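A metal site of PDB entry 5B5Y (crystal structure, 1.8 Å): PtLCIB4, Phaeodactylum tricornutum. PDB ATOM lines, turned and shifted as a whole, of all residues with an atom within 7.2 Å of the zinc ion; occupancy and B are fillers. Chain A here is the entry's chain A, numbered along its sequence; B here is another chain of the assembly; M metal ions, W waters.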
ATOM      1  N   LEU A  60      -1.740   2.877   6.470  1.00  0.00           N
ATOM      2  CA  LEU A  60      -2.562   1.712   6.775  1.00  0.00           C
ATOM      3  C   LEU A  60      -3.681   2.127   7.749  1.00  0.00           C
ATOM      4  O   LEU A  60      -3.570   3.155   8.422  1.00  0.00           O
ATOM      5  CB  LEU A  60      -1.692   0.603   7.370  1.00  0.00           C
ATOM      6  CG  LEU A  60      -0.546   0.077   6.502  1.00  0.00           C
ATOM      7  CD1 LEU A  60       0.341  -0.895   7.288  1.00  0.00           C
ATOM      8  CD2 LEU A  60      -1.062  -0.582   5.238  1.00  0.00           C
ATOM      9  N   CYS A  61      -4.745   1.339   7.814  1.00  0.00           N
ATOM     10  CA  CYS A  61      -5.874   1.703   8.661  1.00  0.00           C
ATOM     11  C   CYS A  61      -5.498   1.804  10.139  1.00  0.00           C
ATOM     12  O   CYS A  61      -4.633   1.073  10.630  1.00  0.00           O
ATOM     13  CB  CYS A  61      -7.027   0.688   8.490  1.00  0.00           C
ATOM     14  SG  CYS A  61      -8.525   1.132   9.419  1.00  0.00           S
ATOM     15  N   SER A  62      -6.149   2.734  10.819  1.00  0.00           N
ATOM     16  CA  SER A  62      -6.101   2.918  12.270  1.00  0.00           C
ATOM     17  C   SER A  62      -6.243   1.649  13.077  1.00  0.00           C
ATOM     18  O   SER A  62      -5.673   1.528  14.160  1.00  0.00           O
ATOM     19  CB  SER A  62      -7.221   3.864  12.666  1.00  0.00           C
ATOM     20  OG  SER A  62      -7.193   5.020  11.858  1.00  0.00           O
ATOM     21  N   ASP A  63      -7.079   0.754  12.572  1.00  0.00           N
ATOM     22  CA  ASP A  63      -7.398  -0.531  13.196  1.00  0.00           C
ATOM     23  C   ASP A  63      -6.149  -1.241  13.719  1.00  0.00           C
ATOM     24  O   ASP A  63      -5.169  -1.361  12.985  1.00  0.00           O
ATOM     25  CB  ASP A  63      -8.139  -1.394  12.157  1.00  0.00           C
ATOM     26  CG  ASP A  63      -8.784  -2.637  12.749  1.00  0.00           C
ATOM     27  OD1 ASP A  63      -8.338  -3.112  13.826  1.00  0.00           O
ATOM     28  OD2 ASP A  63      -9.745  -3.136  12.123  1.00  0.00           O
ATOM     29  N   VAL A  65      -5.422  -4.222  14.121  1.00  0.00           N
ATOM     30  CA  VAL A  65      -4.995  -5.453  13.444  1.00  0.00           C
ATOM     31  C   VAL A  65      -4.043  -5.221  12.260  1.00  0.00           C
ATOM     32  O   VAL A  65      -3.491  -6.163  11.729  1.00  0.00           O
ATOM     33  CB  VAL A  65      -6.196  -6.280  12.924  1.00  0.00           C
ATOM     34  CG1 VAL A  65      -7.077  -6.709  14.090  1.00  0.00           C
ATOM     35  CG2 VAL A  65      -6.979  -5.486  11.885  1.00  0.00           C
ATOM     36  N   THR A  66      -3.818  -3.970  11.881  1.00  0.00           N
ATOM     37  CA  THR A  66      -2.896  -3.709  10.792  1.00  0.00           C
ATOM     38  C   THR A  66      -1.455  -3.488  11.268  1.00  0.00           C
ATOM     39  O   THR A  66      -0.537  -3.470  10.460  1.00  0.00           O
ATOM     40  CB  THR A  66      -3.277  -2.465   9.943  1.00  0.00           C
ATOM     41  OG1 THR A  66      -3.181  -1.286  10.741  1.00  0.00           O
ATOM     42  CG2 THR A  66      -4.682  -2.594   9.374  1.00  0.00           C
ATOM     43  N   GLY A  85      -4.811   6.633   8.332  1.00  0.00           N
ATOM     44  CA  GLY A  85      -6.006   7.080   9.014  1.00  0.00           C
ATOM     45  C   GLY A  85      -7.065   6.053   8.713  1.00  0.00           C
ATOM     46  O   GLY A  85      -6.744   4.934   8.340  1.00  0.00           O
ATOM     47  N   LEU A  86      -8.328   6.431   8.903  1.00  0.00           N
ATOM     48  CA  LEU A  86      -9.425   5.502   8.686  1.00  0.00           C
ATOM     49  C   LEU A  86      -9.386   4.864   7.299  1.00  0.00           C
ATOM     50  O   LEU A  86      -9.222   5.559   6.289  1.00  0.00           O
ATOM     51  CB  LEU A  86     -10.769   6.229   8.872  1.00  0.00           C
ATOM     52  CG  LEU A  86     -11.005   6.823  10.255  1.00  0.00           C
ATOM     53  CD1 LEU A  86     -12.382   7.457  10.332  1.00  0.00           C
ATOM     54  CD2 LEU A  86     -10.848   5.787  11.324  1.00  0.00           C
ATOM     55  N   ALA A  87      -9.501   3.542   7.281  1.00  0.00           N
ATOM     56  CA  ALA A  87      -9.511   2.697   6.074  1.00  0.00           C
ATOM     57  C   ALA A  87      -8.171   2.673   5.327  1.00  0.00           C
ATOM     58  O   ALA A  87      -8.058   2.057   4.272  1.00  0.00           O
ATOM     59  CB  ALA A  87     -10.633   3.126   5.122  1.00  0.00           C
ATOM     60  N   GLY A  88      -7.157   3.316   5.889  1.00  0.00           N
ATOM     61  CA  GLY A  88      -5.834   3.295   5.281  1.00  0.00           C
ATOM     62  C   GLY A  88      -5.541   4.440   4.313  1.00  0.00           C
ATOM     63  O   GLY A  88      -4.472   4.480   3.702  1.00  0.00           O
ATOM     64  N   SER A 116      -5.476  -0.979   1.540  1.00  0.00           N
ATOM     65  CA  SER A 116      -6.720  -1.235   2.244  1.00  0.00           C
ATOM     66  C   SER A 116      -6.500  -2.495   3.061  1.00  0.00           C
ATOM     67  O   SER A 116      -5.462  -3.144   2.945  1.00  0.00           O
ATOM     68  CB  SER A 116      -7.857  -1.460   1.240  1.00  0.00           C
ATOM     69  OG  SER A 116      -7.487  -2.504   0.351  1.00  0.00           O
ATOM     70  N   HIS A 117      -7.467  -2.854   3.875  1.00  0.00           N
ATOM     71  CA  HIS A 117      -7.375  -4.172   4.506  1.00  0.00           C
ATOM     72  C   HIS A 117      -8.731  -4.806   4.660  1.00  0.00           C
ATOM     73  O   HIS A 117      -9.753  -4.155   4.541  1.00  0.00           O
ATOM     74  CB  HIS A 117      -6.664  -4.094   5.856  1.00  0.00           C
ATOM     75  CG  HIS A 117      -7.490  -3.515   6.965  1.00  0.00           C
ATOM     76  ND1 HIS A 117      -7.775  -4.216   8.116  1.00  0.00           N
ATOM     77  CD2 HIS A 117      -8.062  -2.295   7.116  1.00  0.00           C
ATOM     78  CE1 HIS A 117      -8.491  -3.450   8.932  1.00  0.00           C
ATOM     79  NE2 HIS A 117      -8.680  -2.287   8.344  1.00  0.00           N
ATOM     80  N   VAL A 118      -8.722  -6.106   4.951  1.00  0.00           N
ATOM     81  CA  VAL A 118      -9.990  -6.807   5.121  1.00  0.00           C
ATOM     82  C   VAL A 118      -9.722  -7.989   6.036  1.00  0.00           C
ATOM     83  O   VAL A 118      -8.650  -8.575   5.994  1.00  0.00           O
ATOM     84  CB  VAL A 118     -10.576  -7.282   3.767  1.00  0.00           C
ATOM     85  CG1 VAL A 118      -9.648  -8.249   3.059  1.00  0.00           C
ATOM     86  CG2 VAL A 118     -11.944  -7.931   3.985  1.00  0.00           C
ATOM     87  N   ARG A 131     -11.273 -11.086  17.033  1.00  0.00           N
ATOM     88  CA  ARG A 131     -10.394 -10.143  17.713  1.00  0.00           C
ATOM     89  C   ARG A 131     -10.099 -10.611  19.137  1.00  0.00           C
ATOM     90  O   ARG A 131     -10.978 -11.169  19.794  1.00  0.00           O
ATOM     91  CB  ARG A 131     -11.017  -8.746  17.731  1.00  0.00           C
ATOM     92  CG  ARG A 131     -11.307  -8.187  16.350  1.00  0.00           C
ATOM     93  CD  ARG A 131     -11.828  -6.752  16.400  1.00  0.00           C
ATOM     94  NE  ARG A 131     -12.013  -6.226  15.049  1.00  0.00           N
ATOM     95  CZ  ARG A 131     -11.145  -5.462  14.408  1.00  0.00           C
ATOM     96  NH1 ARG A 131     -10.023  -5.072  15.011  1.00  0.00           N
ATOM     97  NH2 ARG A 131     -11.411  -5.045  13.172  1.00  0.00           N
ATOM     98  N   ALA A 139     -16.946  -5.789  12.215  1.00  0.00           N
ATOM     99  CA  ALA A 139     -16.463  -5.558  10.859  1.00  0.00           C
ATOM    100  C   ALA A 139     -14.964  -5.291  10.811  1.00  0.00           C
ATOM    101  O   ALA A 139     -14.367  -4.769  11.752  1.00  0.00           O
ATOM    102  CB  ALA A 139     -17.219  -4.408  10.212  1.00  0.00           C
ATOM    103  N   CYS A 140     -14.366  -5.624   9.676  1.00  0.00           N
ATOM    104  CA  CYS A 140     -12.953  -5.393   9.397  1.00  0.00           C
ATOM    105  C   CYS A 140     -12.833  -5.381   7.850  1.00  0.00           C
ATOM    106  O   CYS A 140     -12.935  -6.376   7.290  1.00  0.00           O
ATOM    107  CB  CYS A 140     -12.077  -6.495   9.961  1.00  0.00           C
ATOM    108  SG  CYS A 140     -10.282  -6.358   9.717  1.00  0.00           S
ATOM    109  N   CYS A 141     -12.667  -4.236   7.202  1.00  0.00           N
ATOM    110  CA  CYS A 141     -12.521  -2.902   7.743  1.00  0.00           C
ATOM    111  C   CYS A 141     -13.813  -2.173   8.120  1.00  0.00           C
ATOM    112  O   CYS A 141     -14.630  -1.957   7.346  1.00  0.00           O
ATOM    113  CB  CYS A 141     -11.698  -2.076   6.747  1.00  0.00           C
ATOM    114  SG  CYS A 141     -11.425  -0.295   7.028  1.00  0.00           S
ATOM    115  N   GLY A 142     -13.892  -1.861   9.398  1.00  0.00           N
ATOM    116  CA  GLY A 142     -15.013  -1.188   9.966  1.00  0.00           C
ATOM    117  C   GLY A 142     -15.353   0.108   9.271  1.00  0.00           C
ATOM    118  O   GLY A 142     -16.446   0.322   8.846  1.00  0.00           O
ATOM    119  N   SER A 143     -14.350   0.963   9.166  1.00  0.00           N
ATOM    120  CA  SER A 143     -14.538   2.245   8.479  1.00  0.00           C
ATOM    121  C   SER A 143     -15.043   2.040   7.055  1.00  0.00           C
ATOM    122  O   SER A 143     -16.014   2.690   6.625  1.00  0.00           O
ATOM    123  CB  SER A 143     -13.221   3.043   8.471  1.00  0.00           C
ATOM    124  OG  SER A 143     -13.335   4.181   7.618  1.00  0.00           O
ATOM    125  N   ALA A 144     -14.371   1.180   6.304  1.00  0.00           N
ATOM    126  CA  ALA A 144     -14.752   0.960   4.911  1.00  0.00           C
ATOM    127  C   ALA A 144     -16.161   0.375   4.789  1.00  0.00           C
ATOM    128  O   ALA A 144     -16.927   0.776   3.918  1.00  0.00           O
ATOM    129  CB  ALA A 144     -13.729   0.058   4.207  1.00  0.00           C
ATOM    130  N   ASN A 249      -6.184  -9.617   6.921  1.00  0.00           N
ATOM    131  CA  ASN A 249      -6.043  -9.916   8.340  1.00  0.00           C
ATOM    132  C   ASN A 249      -6.792 -11.193   8.715  1.00  0.00           C
ATOM    133  O   ASN A 249      -8.016 -11.290   8.615  1.00  0.00           O
ATOM    134  CB  ASN A 249      -6.545  -8.738   9.199  1.00  0.00           C
ATOM    135  CG  ASN A 249      -5.784  -7.445   8.886  1.00  0.00           C
ATOM    136  OD1 ASN A 249      -6.380  -6.432   8.506  1.00  0.00           O
ATOM    137  ND2 ASN A 249      -4.455  -7.495   9.019  1.00  0.00           N
ATOM    138  N   PHE B  81      -4.453   0.823  18.608  1.00  0.00           N
ATOM    139  CA  PHE B  81      -5.298   1.501  17.641  1.00  0.00           C
ATOM    140  C   PHE B  81      -4.752   2.919  17.501  1.00  0.00           C
ATOM    141  O   PHE B  81      -4.393   3.530  18.497  1.00  0.00           O
ATOM    142  CB  PHE B  81      -6.747   1.500  18.141  1.00  0.00           C
ATOM    143  CG  PHE B  81      -7.723   2.073  17.178  1.00  0.00           C
ATOM    144  CD1 PHE B  81      -7.853   3.439  17.043  1.00  0.00           C
ATOM    145  CD2 PHE B  81      -8.549   1.251  16.427  1.00  0.00           C
ATOM    146  CE1 PHE B  81      -8.761   3.983  16.174  1.00  0.00           C
ATOM    147  CE2 PHE B  81      -9.462   1.787  15.552  1.00  0.00           C
ATOM    148  CZ  PHE B  81      -9.569   3.158  15.410  1.00  0.00           C
ATOM    149  N   HIS B 103     -13.569  -2.786  19.514  1.00  0.00           N
ATOM    150  CA  HIS B 103     -12.462  -3.697  19.518  1.00  0.00           C
ATOM    151  C   HIS B 103     -12.001  -4.051  20.972  1.00  0.00           C
ATOM    152  O   HIS B 103     -11.167  -4.863  21.139  1.00  0.00           O
ATOM    153  CB  HIS B 103     -11.254  -3.110  18.798  1.00  0.00           C
ATOM    154  CG  HIS B 103     -11.469  -2.788  17.355  1.00  0.00           C
ATOM    155  ND1 HIS B 103     -12.578  -3.164  16.651  1.00  0.00           N
ATOM    156  CD2 HIS B 103     -10.675  -2.135  16.478  1.00  0.00           C
ATOM    157  CE1 HIS B 103     -12.468  -2.741  15.398  1.00  0.00           C
ATOM    158  NE2 HIS B 103     -11.328  -2.113  15.279  1.00  0.00           N
HETATM  159 ZN    ZN M   1      -9.888  -0.600   8.853  1.00  0.00          ZN
HETATM  160  O   HOH W   1     -10.878  -1.363  10.426  1.00  0.00           O
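The zinc ion is bound by water W1 (2.0 Å). NE2 of His 117 binds the zinc ion, 2.1 Å away. The side-chain sulfur (SG) of Cys 61 binds the zinc ion, at 2.3 Å. SG of Cys 141 binds the zinc ion (2.4 Å). The zinc ion has four donor atoms within binding distance.
Water W1 bridges the side-chain carboxylate (OD2) of Asp 63 (2.7 Å) and the backbone NH (N) of Gly 142 (3.2 Å).
SG of Cys 61 sits close to N of Asp 63, at 3.5 Å. N of Val 65 lies close to OD1 of Asp 63. The side-chain amide oxygen (OD1) of Asn 249 lies within hydrogen-bond range of a ring nitrogen (ND1) of His 117 (2.6 Å). The backbone carbonyl oxygen of Cys 61 lies within hydrogen-bond range of the side-chain hydroxyl of Thr 66 (2.8 Å). The side-chain hydroxyl (OG1) of Thr 66 lies within hydrogen-bond range of the backbone carbonyl oxygen (O) of Asp 63 (3.0 Å). The side-chain carboxylate (OD1) of Asp 63 lies within hydrogen-bond range of a ring nitrogen (NE2) of His 103 of chain B, at 3.5 Å. The side-chain sulfur (SG) of Cys 61 lies close to the backbone NH (N) of Ala 87, at 3.4 Å. SG of Cys 140 sits close to ND1 of His 117 (3.7 Å).
Residues that only touch the zinc ion: Asp 63. Within 4 Å of the zinc ion: Cys 61, Asp 63, His 117 and Cys 141.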
